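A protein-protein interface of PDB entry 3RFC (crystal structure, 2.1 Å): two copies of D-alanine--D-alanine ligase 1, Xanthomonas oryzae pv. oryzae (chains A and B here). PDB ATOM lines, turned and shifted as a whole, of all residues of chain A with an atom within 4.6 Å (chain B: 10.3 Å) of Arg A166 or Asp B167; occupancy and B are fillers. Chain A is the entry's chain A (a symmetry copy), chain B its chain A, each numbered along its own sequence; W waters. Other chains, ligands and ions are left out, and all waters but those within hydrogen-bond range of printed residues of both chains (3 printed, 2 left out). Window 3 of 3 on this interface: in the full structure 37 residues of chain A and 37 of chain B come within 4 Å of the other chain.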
ATOM      1  N   LYS A 162       6.744   1.966   7.869  1.00  0.00           N
ATOM      2  CA  LYS A 162       7.845   2.028   8.872  1.00  0.00           C
ATOM      3  C   LYS A 162       7.430   2.641  10.176  1.00  0.00           C
ATOM      4  O   LYS A 162       7.867   2.182  11.253  1.00  0.00           O
ATOM      5  CB  LYS A 162       9.058   2.797   8.305  1.00  0.00           C
ATOM      6  CG  LYS A 162       9.859   1.999   7.282  1.00  0.00           C
ATOM      7  CD  LYS A 162      10.772   2.932   6.550  1.00  0.00           C
ATOM      8  CE  LYS A 162      11.989   2.222   6.007  1.00  0.00           C
ATOM      9  NZ  LYS A 162      13.119   2.395   6.941  1.00  0.00           N
ATOM     10  N   ARG A 163       6.566   3.661  10.125  1.00  0.00           N
ATOM     11  CA  ARG A 163       6.044   4.200  11.384  1.00  0.00           C
ATOM     12  C   ARG A 163       5.186   3.192  12.127  1.00  0.00           C
ATOM     13  O   ARG A 163       5.280   3.123  13.382  1.00  0.00           O
ATOM     14  CB  ARG A 163       5.364   5.556  11.222  1.00  0.00           C
ATOM     15  CG  ARG A 163       6.362   6.674  10.737  1.00  0.00           C
ATOM     16  CD  ARG A 163       5.675   8.041  10.591  1.00  0.00           C
ATOM     17  NE  ARG A 163       4.957   8.201   9.328  1.00  0.00           N
ATOM     18  CZ  ARG A 163       3.695   8.615   9.192  1.00  0.00           C
ATOM     19  NH1 ARG A 163       2.906   8.854  10.256  1.00  0.00           N
ATOM     20  NH2 ARG A 163       3.217   8.780   7.966  1.00  0.00           N
ATOM     21  N   VAL A 164       4.348   2.426  11.409  1.00  0.00           N
ATOM     22  CA  VAL A 164       3.510   1.425  12.093  1.00  0.00           C
ATOM     23  C   VAL A 164       4.394   0.260  12.629  1.00  0.00           C
ATOM     24  O   VAL A 164       4.165  -0.253  13.741  1.00  0.00           O
ATOM     25  CB  VAL A 164       2.424   0.826  11.199  1.00  0.00           C
ATOM     26  CG1 VAL A 164       1.652  -0.230  12.004  1.00  0.00           C
ATOM     27  CG2 VAL A 164       1.453   1.933  10.756  1.00  0.00           C
ATOM     28  N   LEU A 165       5.391  -0.125  11.848  1.00  0.00           N
ATOM     29  CA  LEU A 165       6.401  -1.151  12.264  1.00  0.00           C
ATOM     30  C   LEU A 165       7.184  -0.724  13.497  1.00  0.00           C
ATOM     31  O   LEU A 165       7.385  -1.514  14.418  1.00  0.00           O
ATOM     32  CB  LEU A 165       7.382  -1.431  11.120  1.00  0.00           C
ATOM     33  CG  LEU A 165       6.642  -2.223  10.003  1.00  0.00           C
ATOM     34  CD1 LEU A 165       7.554  -2.521   8.817  1.00  0.00           C
ATOM     35  CD2 LEU A 165       5.996  -3.518  10.518  1.00  0.00           C
ATOM     36  N   ARG A 166       7.591   0.544  13.485  1.00  0.00           N
ATOM     37  CA  ARG A 166       8.333   1.171  14.553  1.00  0.00           C
ATOM     38  C   ARG A 166       7.566   1.130  15.855  1.00  0.00           C
ATOM     39  O   ARG A 166       8.139   0.774  16.882  1.00  0.00           O
ATOM     40  CB  ARG A 166       8.700   2.646  14.174  1.00  0.00           C
ATOM     41  CG  ARG A 166       9.518   3.365  15.249  1.00  0.00           C
ATOM     42  CD  ARG A 166      10.194   4.649  14.696  1.00  0.00           C
ATOM     43  NE  ARG A 166       9.212   5.667  14.355  1.00  0.00           N
ATOM     44  CZ  ARG A 166       9.436   6.722  13.580  1.00  0.00           C
ATOM     45  NH1 ARG A 166      10.611   6.918  12.995  1.00  0.00           N
ATOM     46  NH2 ARG A 166       8.458   7.585  13.392  1.00  0.00           N
ATOM     47  N   ASP A 167       6.290   1.527  15.799  1.00  0.00           N
ATOM     48  CA  ASP A 167       5.390   1.555  16.944  1.00  0.00           C
ATOM     49  C   ASP A 167       5.177   0.143  17.445  1.00  0.00           C
ATOM     50  O   ASP A 167       4.949  -0.079  18.629  1.00  0.00           O
ATOM     51  CB  ASP A 167       4.038   2.106  16.509  1.00  0.00           C
ATOM     52  CG  ASP A 167       3.011   2.176  17.644  1.00  0.00           C
ATOM     53  OD1 ASP A 167       3.097   3.077  18.513  1.00  0.00           O
ATOM     54  OD2 ASP A 167       2.081   1.342  17.637  1.00  0.00           O
ATOM     55  N   ALA A 168       5.217  -0.824  16.547  1.00  0.00           N
ATOM     56  CA  ALA A 168       5.052  -2.224  16.963  1.00  0.00           C
ATOM     57  C   ALA A 168       6.347  -2.776  17.580  1.00  0.00           C
ATOM     58  O   ALA A 168       6.453  -3.991  17.764  1.00  0.00           O
ATOM     59  CB  ALA A 168       4.673  -3.097  15.775  1.00  0.00           C
ATOM     60  N   ARG A 169       7.338  -1.913  17.824  1.00  0.00           N
ATOM     61  CA  ARG A 169       8.651  -2.358  18.346  1.00  0.00           C
ATOM     62  C   ARG A 169       9.371  -3.359  17.452  1.00  0.00           C
ATOM     63  O   ARG A 169      10.122  -4.197  17.940  1.00  0.00           O
ATOM     64  CB  ARG A 169       8.481  -2.987  19.739  1.00  0.00           C
ATOM     65  CG  ARG A 169       7.853  -2.025  20.761  1.00  0.00           C
ATOM     66  CD  ARG A 169       8.760  -0.800  20.778  1.00  0.00           C
ATOM     67  NE  ARG A 169       8.534  -0.001  21.974  1.00  0.00           N
ATOM     68  CZ  ARG A 169       7.635   0.976  22.068  1.00  0.00           C
ATOM     69  NH1 ARG A 169       6.874   1.302  21.015  1.00  0.00           N
ATOM     70  NH2 ARG A 169       7.511   1.630  23.218  1.00  0.00           N
ATOM     71  N   LEU A 170       9.123  -3.310  16.147  1.00  0.00           N
ATOM     72  CA  LEU A 170       9.986  -4.022  15.245  1.00  0.00           C
ATOM     73  C   LEU A 170      11.005  -3.038  14.696  1.00  0.00           C
ATOM     74  O   LEU A 170      10.671  -1.856  14.494  1.00  0.00           O
ATOM     75  CB  LEU A 170       9.169  -4.638  14.110  1.00  0.00           C
ATOM     76  CG  LEU A 170       8.155  -5.635  14.658  1.00  0.00           C
ATOM     77  CD1 LEU A 170       6.909  -5.793  13.831  1.00  0.00           C
ATOM     78  CD2 LEU A 170       8.820  -6.983  15.068  1.00  0.00           C
ATOM     79  N   PHE A 175      15.426   6.570   9.650  1.00  0.00           N
ATOM     80  CA  PHE A 175      15.041   7.258   8.429  1.00  0.00           C
ATOM     81  C   PHE A 175      14.387   8.606   8.664  1.00  0.00           C
ATOM     82  O   PHE A 175      13.839   8.855   9.723  1.00  0.00           O
ATOM     83  CB  PHE A 175      14.050   6.378   7.613  1.00  0.00           C
ATOM     84  CG  PHE A 175      12.661   6.404   8.162  1.00  0.00           C
ATOM     85  CD1 PHE A 175      11.727   7.326   7.686  1.00  0.00           C
ATOM     86  CD2 PHE A 175      12.288   5.523   9.166  1.00  0.00           C
ATOM     87  CE1 PHE A 175      10.421   7.345   8.181  1.00  0.00           C
ATOM     88  CE2 PHE A 175      11.002   5.509   9.668  1.00  0.00           C
ATOM     89  CZ  PHE A 175      10.047   6.444   9.175  1.00  0.00           C
ATOM     90  N   ASP B 159      -7.806   1.695  15.854  1.00  0.00           N
ATOM     91  CA  ASP B 159      -6.637   1.046  16.320  1.00  0.00           C
ATOM     92  C   ASP B 159      -5.395   1.566  15.576  1.00  0.00           C
ATOM     93  O   ASP B 159      -4.476   2.125  16.195  1.00  0.00           O
ATOM     94  CB  ASP B 159      -6.779  -0.495  16.185  1.00  0.00           C
ATOM     95  CG  ASP B 159      -5.484  -1.209  16.326  1.00  0.00           C
ATOM     96  OD1 ASP B 159      -4.747  -0.934  17.292  1.00  0.00           O
ATOM     97  OD2 ASP B 159      -5.191  -2.052  15.450  1.00  0.00           O
ATOM     98  N   MET B 160      -5.393   1.432  14.262  1.00  0.00           N
ATOM     99  CA  MET B 160      -4.257   1.902  13.427  1.00  0.00           C
ATOM    100  C   MET B 160      -4.052   3.425  13.665  1.00  0.00           C
ATOM    101  O   MET B 160      -2.937   3.896  13.817  1.00  0.00           O
ATOM    102  CB  MET B 160      -4.651   1.667  11.956  1.00  0.00           C
ATOM    103  CG  MET B 160      -3.574   1.931  10.967  1.00  0.00           C
ATOM    104  SD  MET B 160      -2.145   0.856  11.123  1.00  0.00           S
ATOM    105  CE  MET B 160      -2.731  -0.778  10.565  1.00  0.00           C
ATOM    106  N   ALA B 161      -5.136   4.172  13.678  1.00  0.00           N
ATOM    107  CA  ALA B 161      -5.051   5.634  13.871  1.00  0.00           C
ATOM    108  C   ALA B 161      -4.320   6.007  15.150  1.00  0.00           C
ATOM    109  O   ALA B 161      -3.446   6.817  15.108  1.00  0.00           O
ATOM    110  CB  ALA B 161      -6.445   6.305  13.832  1.00  0.00           C
ATOM    111  N   LYS B 162      -4.693   5.383  16.265  1.00  0.00           N
ATOM    112  CA  LYS B 162      -4.012   5.613  17.571  1.00  0.00           C
ATOM    113  C   LYS B 162      -2.581   5.166  17.584  1.00  0.00           C
ATOM    114  O   LYS B 162      -1.720   5.837  18.190  1.00  0.00           O
ATOM    115  CB  LYS B 162      -4.780   4.917  18.717  1.00  0.00           C
ATOM    116  CG  LYS B 162      -6.065   5.635  19.113  1.00  0.00           C
ATOM    117  CD  LYS B 162      -6.890   4.717  19.957  1.00  0.00           C
ATOM    118  CE  LYS B 162      -7.814   5.475  20.880  1.00  0.00           C
ATOM    119  NZ  LYS B 162      -7.193   5.588  22.215  1.00  0.00           N
ATOM    120  N   ARG B 163      -2.281   4.054  16.904  1.00  0.00           N
ATOM    121  CA  ARG B 163      -0.874   3.659  16.792  1.00  0.00           C
ATOM    122  C   ARG B 163      -0.060   4.661  15.992  1.00  0.00           C
ATOM    123  O   ARG B 163       1.108   4.935  16.373  1.00  0.00           O
ATOM    124  CB  ARG B 163      -0.688   2.223  16.314  1.00  0.00           C
ATOM    125  CG  ARG B 163      -1.277   1.172  17.328  1.00  0.00           C
ATOM    126  CD  ARG B 163      -1.073  -0.274  16.850  1.00  0.00           C
ATOM    127  NE  ARG B 163      -2.077  -0.717  15.883  1.00  0.00           N
ATOM    128  CZ  ARG B 163      -1.827  -1.296  14.706  1.00  0.00           C
ATOM    129  NH1 ARG B 163      -0.574  -1.459  14.244  1.00  0.00           N
ATOM    130  NH2 ARG B 163      -2.856  -1.707  13.979  1.00  0.00           N
ATOM    131  N   VAL B 164      -0.623   5.197  14.896  1.00  0.00           N
ATOM    132  CA  VAL B 164       0.130   6.184  14.101  1.00  0.00           C
ATOM    133  C   VAL B 164       0.272   7.517  14.894  1.00  0.00           C
ATOM    134  O   VAL B 164       1.335   8.166  14.863  1.00  0.00           O
ATOM    135  CB  VAL B 164      -0.516   6.500  12.752  1.00  0.00           C
ATOM    136  CG1 VAL B 164       0.328   7.567  12.041  1.00  0.00           C
ATOM    137  CG2 VAL B 164      -0.552   5.228  11.888  1.00  0.00           C
ATOM    138  N   LEU B 165      -0.783   7.892  15.601  1.00  0.00           N
ATOM    139  CA  LEU B 165      -0.772   9.086  16.508  1.00  0.00           C
ATOM    140  C   LEU B 165       0.256   8.955  17.622  1.00  0.00           C
ATOM    141  O   LEU B 165       0.991   9.899  17.912  1.00  0.00           O
ATOM    142  CB  LEU B 165      -2.157   9.300  17.127  1.00  0.00           C
ATOM    143  CG  LEU B 165      -3.130   9.812  16.025  1.00  0.00           C
ATOM    144  CD1 LEU B 165      -4.539  10.028  16.567  1.00  0.00           C
ATOM    145  CD2 LEU B 165      -2.625  11.083  15.328  1.00  0.00           C
ATOM    146  N   ARG B 166       0.292   7.760  18.207  1.00  0.00           N
ATOM    147  CA  ARG B 166       1.198   7.401  19.273  1.00  0.00           C
ATOM    148  C   ARG B 166       2.639   7.553  18.846  1.00  0.00           C
ATOM    149  O   ARG B 166       3.431   8.133  19.587  1.00  0.00           O
ATOM    150  CB  ARG B 166       0.918   5.942  19.764  1.00  0.00           C
ATOM    151  CG  ARG B 166       1.820   5.504  20.920  1.00  0.00           C
ATOM    152  CD  ARG B 166       1.270   4.240  21.636  1.00  0.00           C
ATOM    153  NE  ARG B 166       1.323   3.070  20.772  1.00  0.00           N
ATOM    154  CZ  ARG B 166       0.650   1.943  20.965  1.00  0.00           C
ATOM    155  NH1 ARG B 166      -0.194   1.799  21.981  1.00  0.00           N
ATOM    156  NH2 ARG B 166       0.829   0.947  20.119  1.00  0.00           N
ATOM    157  N   ASP B 167       2.967   7.001  17.673  1.00  0.00           N
ATOM    158  CA  ASP B 167       4.302   7.044  17.091  1.00  0.00           C
ATOM    159  C   ASP B 167       4.666   8.481  16.787  1.00  0.00           C
ATOM    160  O   ASP B 167       5.834   8.857  16.818  1.00  0.00           O
ATOM    161  CB  ASP B 167       4.304   6.273  15.778  1.00  0.00           C
ATOM    162  CG  ASP B 167       5.668   6.257  15.079  1.00  0.00           C
ATOM    163  OD1 ASP B 167       6.586   5.521  15.512  1.00  0.00           O
ATOM    164  OD2 ASP B 167       5.803   6.961  14.055  1.00  0.00           O
ATOM    165  N   ALA B 168       3.678   9.293  16.456  1.00  0.00           N
ATOM    166  CA  ALA B 168       3.951  10.711  16.179  1.00  0.00           C
ATOM    167  C   ALA B 168       4.137  11.505  17.482  1.00  0.00           C
ATOM    168  O   ALA B 168       4.138  12.738  17.437  1.00  0.00           O
ATOM    169  CB  ALA B 168       2.806  11.334  15.394  1.00  0.00           C
ATOM    170  N   ARG B 169       4.217  10.817  18.625  1.00  0.00           N
ATOM    171  CA  ARG B 169       4.321  11.494  19.938  1.00  0.00           C
ATOM    172  C   ARG B 169       3.156  12.423  20.256  1.00  0.00           C
ATOM    173  O   ARG B 169       3.326  13.412  20.961  1.00  0.00           O
ATOM    174  CB  ARG B 169       5.623  12.308  20.014  1.00  0.00           C
ATOM    175  CG  ARG B 169       6.882  11.449  19.809  1.00  0.00           C
ATOM    176  CD  ARG B 169       6.810  10.361  20.873  1.00  0.00           C
ATOM    177  NE  ARG B 169       8.111   9.738  21.071  1.00  0.00           N
ATOM    178  CZ  ARG B 169       8.554   8.687  20.385  1.00  0.00           C
ATOM    179  NH1 ARG B 169       7.783   8.109  19.454  1.00  0.00           N
ATOM    180  NH2 ARG B 169       9.766   8.210  20.646  1.00  0.00           N
ATOM    181  N   LEU B 170       1.977  12.140  19.712  1.00  0.00           N
ATOM    182  CA  LEU B 170       0.802  12.801  20.209  1.00  0.00           C
ATOM    183  C   LEU B 170       0.129  11.873  21.208  1.00  0.00           C
ATOM    184  O   LEU B 170       0.165  10.642  21.025  1.00  0.00           O
ATOM    185  CB  LEU B 170      -0.147  13.128  19.058  1.00  0.00           C
ATOM    186  CG  LEU B 170       0.521  14.068  18.062  1.00  0.00           C
ATOM    187  CD1 LEU B 170       0.035  13.943  16.644  1.00  0.00           C
ATOM    188  CD2 LEU B 170       0.578  15.534  18.586  1.00  0.00           C
ATOM    189  N   ALA B 171      -0.536  12.463  22.210  1.00  0.00           N
ATOM    190  CA  ALA B 171      -1.168  11.710  23.300  1.00  0.00           C
ATOM    191  C   ALA B 171      -2.490  11.129  22.795  1.00  0.00           C
ATOM    192  O   ALA B 171      -3.285  11.848  22.149  1.00  0.00           O
ATOM    193  CB  ALA B 171      -1.479  12.630  24.473  1.00  0.00           C
ATOM    194  N   VAL B 172      -2.744   9.864  23.108  1.00  0.00           N
ATOM    195  CA  VAL B 172      -4.098   9.299  22.874  1.00  0.00           C
ATOM    196  C   VAL B 172      -4.399   8.543  24.177  1.00  0.00           C
ATOM    197  O   VAL B 172      -3.500   8.358  24.966  1.00  0.00           O
ATOM    198  CB  VAL B 172      -4.098   8.323  21.722  1.00  0.00           C
ATOM    199  CG1 VAL B 172      -3.915   9.063  20.400  1.00  0.00           C
ATOM    200  CG2 VAL B 172      -2.971   7.288  21.936  1.00  0.00           C
ATOM    201  N   PHE B 175      -4.695   2.199  25.732  1.00  0.00           N
ATOM    202  CA  PHE B 175      -5.680   1.287  25.176  1.00  0.00           C
ATOM    203  C   PHE B 175      -5.122  -0.077  24.818  1.00  0.00           C
ATOM    204  O   PHE B 175      -3.935  -0.220  24.587  1.00  0.00           O
ATOM    205  CB  PHE B 175      -6.310   1.902  23.893  1.00  0.00           C
ATOM    206  CG  PHE B 175      -5.419   1.794  22.699  1.00  0.00           C
ATOM    207  CD1 PHE B 175      -5.520   0.704  21.834  1.00  0.00           C
ATOM    208  CD2 PHE B 175      -4.467   2.770  22.446  1.00  0.00           C
ATOM    209  CE1 PHE B 175      -4.703   0.604  20.706  1.00  0.00           C
ATOM    210  CE2 PHE B 175      -3.652   2.708  21.332  1.00  0.00           C
ATOM    211  CZ  PHE B 175      -3.763   1.598  20.446  1.00  0.00           C
ATOM    212  N   GLN B 305      -0.878  18.586  13.265  1.00  0.00           N
ATOM    213  CA  GLN B 305       0.089  17.465  13.349  1.00  0.00           C
ATOM    214  C   GLN B 305      -0.573  16.056  13.255  1.00  0.00           C
ATOM    215  O   GLN B 305      -0.056  15.183  12.548  1.00  0.00           O
ATOM    216  CB  GLN B 305       0.779  17.485  14.704  1.00  0.00           C
ATOM    217  CG  GLN B 305       1.879  18.518  14.947  1.00  0.00           C
ATOM    218  CD  GLN B 305       2.328  18.460  16.434  1.00  0.00           C
ATOM    219  OE1 GLN B 305       1.660  19.020  17.318  1.00  0.00           O
ATOM    220  NE2 GLN B 305       3.416  17.728  16.709  1.00  0.00           N
ATOM    221  N   ALA B 306      -1.668  15.856  13.984  1.00  0.00           N
ATOM    222  CA  ALA B 306      -2.472  14.617  13.904  1.00  0.00           C
ATOM    223  C   ALA B 306      -2.923  14.375  12.449  1.00  0.00           C
ATOM    224  O   ALA B 306      -2.716  13.303  11.905  1.00  0.00           O
ATOM    225  CB  ALA B 306      -3.734  14.734  14.796  1.00  0.00           C
ATOM    226  N   GLN B 308      -1.633  15.584   9.635  1.00  0.00           N
ATOM    227  CA  GLN B 308      -0.434  15.202   8.833  1.00  0.00           C
ATOM    228  C   GLN B 308       0.022  13.779   9.054  1.00  0.00           C
ATOM    229  O   GLN B 308       0.237  13.026   8.103  1.00  0.00           O
ATOM    230  CB  GLN B 308       0.696  16.225   9.024  1.00  0.00           C
ATOM    231  CG  GLN B 308       0.170  17.544   8.411  1.00  0.00           C
ATOM    232  CD  GLN B 308       1.179  18.634   8.271  1.00  0.00           C
ATOM    233  OE1 GLN B 308       1.825  18.996   9.245  1.00  0.00           O
ATOM    234  NE2 GLN B 308       1.282  19.217   7.041  1.00  0.00           N
ATOM    235  N   ALA B 309       0.049  13.375  10.309  1.00  0.00           N
ATOM    236  CA  ALA B 309       0.549  12.050  10.685  1.00  0.00           C
ATOM    237  C   ALA B 309      -0.284  10.901  10.045  1.00  0.00           C
ATOM    238  O   ALA B 309       0.278   9.896   9.611  1.00  0.00           O
ATOM    239  CB  ALA B 309       0.579  11.947  12.252  1.00  0.00           C
ATOM    240  N   LEU B 310      -1.589  11.086   9.968  1.00  0.00           N
ATOM    241  CA  LEU B 310      -2.528  10.069   9.445  1.00  0.00           C
ATOM    242  C   LEU B 310      -2.701  10.172   7.902  1.00  0.00           C
ATOM    243  O   LEU B 310      -3.273   9.293   7.292  1.00  0.00           O
ATOM    244  CB  LEU B 310      -3.887  10.194  10.116  1.00  0.00           C
ATOM    245  CG  LEU B 310      -3.877  10.125  11.646  1.00  0.00           C
ATOM    246  CD1 LEU B 310      -5.204  10.454  12.235  1.00  0.00           C
ATOM    247  CD2 LEU B 310      -3.463   8.773  12.048  1.00  0.00           C
ATOM    248  N   ILE B 330      -5.833  13.287  22.113  1.00  0.00           N
ATOM    249  CA  ILE B 330      -6.660  13.122  20.923  1.00  0.00           C
ATOM    250  C   ILE B 330      -7.619  11.963  21.079  1.00  0.00           C
ATOM    251  O   ILE B 330      -7.197  10.831  21.249  1.00  0.00           O
ATOM    252  CB  ILE B 330      -5.825  12.880  19.661  1.00  0.00           C
ATOM    253  CG1 ILE B 330      -4.956  14.107  19.342  1.00  0.00           C
ATOM    254  CG2 ILE B 330      -6.760  12.567  18.473  1.00  0.00           C
ATOM    255  CD1 ILE B 330      -3.724  13.743  18.523  1.00  0.00           C
HETATM  256  O   HOH W   1       1.487  10.828   6.890  1.00  0.00           O
HETATM  257  O   HOH W   2       1.788  -0.700  15.424  1.00  0.00           O
HETATM  258  O   HOH W   3       3.513   8.581  12.921  1.00  0.00           O
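Hydrophobic or aromatic side chains of chain B within 4 Å of the printed part of chain A: Met B160 and Val B164. Hydrophobic or aromatic side chains of chain A that line the printed part of chain B: Val A164. Among the printed residues, Asp or Glu carboxylates within 4 Å of a Lys or Arg side-chain nitrogen of the other chain: Arg A166 with Asp B167 and Asp A167 with Arg B166.
Water W3 lies within hydrogen-bond range of NH1 of Arg A163, O of Val B164 and OD2 of Asp B167. Water W2 lies within hydrogen-bond range of the guanidinium group of Arg B163, the backbone carbonyl oxygen of Val A164 and the side-chain carboxylate of Asp A167. Water W1 lies within hydrogen-bond range of O of Gln B308 (2.8 Å), NH2 of Arg A163 (2.9 Å) and O of Ala B309 (3.1 Å).
Arg A163 touches Val B164, and with the chains exchanged Val A164 touches Arg B163. Arg A163 touches Asp B167, and with the chains exchanged Asp A167 touches Arg B163. Arg A166 touches Asp B167, and with the chains exchanged Asp A167 touches Arg B166.
Of the printed residues of chain B, Arg A163 touches Val B164 (3.4 Å), Asp B167 (3.2 Å) and Ala B309 (2.9 Å). No residue of chain B comes within 4 Å of Leu A165. Arg A166 touches one residue of chain B. No residue of chain B comes within 4 Å of Ala A168. Of the printed residues of chain A, Met B160 touches Val A164 (3.8 Å). Of the printed residues of chain A, Arg B163 touches Val A164 and Asp A167. Of the printed residues of chain A, Val B164 touches Arg A163 (3.4 Å). Of the printed residues of chain A, Asp B167 touches Arg A163 (3.2 Å) and Arg A166 (2.8 Å). The nearest residue of chain B that does not touch Arg A166 is Arg B169 (5.8 Å).
The side-chain carboxylate (OD1) of Asp A167 lies close to the backbone carbonyl oxygen (O) of Arg B163 (3.5 Å). NH2 of Arg B166 lies within salt-bridge range of OD2 of Asp A167 (2.8 Å). O of Ala B309 sits at hydrogen-bond distance from NH1 of Arg A163, at 2.9 Å. OD2 of Asp B167 is in salt-bridge range of NH2 of Arg A166 (2.8 Å). O of Arg A163 lies close to OD1 of Asp B167, at 3.5 Å.
The backbone carbonyl oxygen of Asp B167 lies within hydrogen-bond range of the guanidinium group of Arg B169 (3.4 Å). The backbone carbonyl oxygen (O) of Asp A167 is in hydrogen-bond range of the guanidinium group (NH1) of Arg A169, at 3.4 Å. The side-chain carboxylate (OD2) of Asp B159 is in salt-bridge range of the guanidinium group (NH2) of Arg B163, at 2.8 Å.
NH1 of Arg A163 touches CG1 of Val B164, 3.4 Å away. Met B160 touches Val A164 (SD to CG2, 3.8 Å). CG1 of Val A164 touches NH1 of Arg B163, 3.4 Å away.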
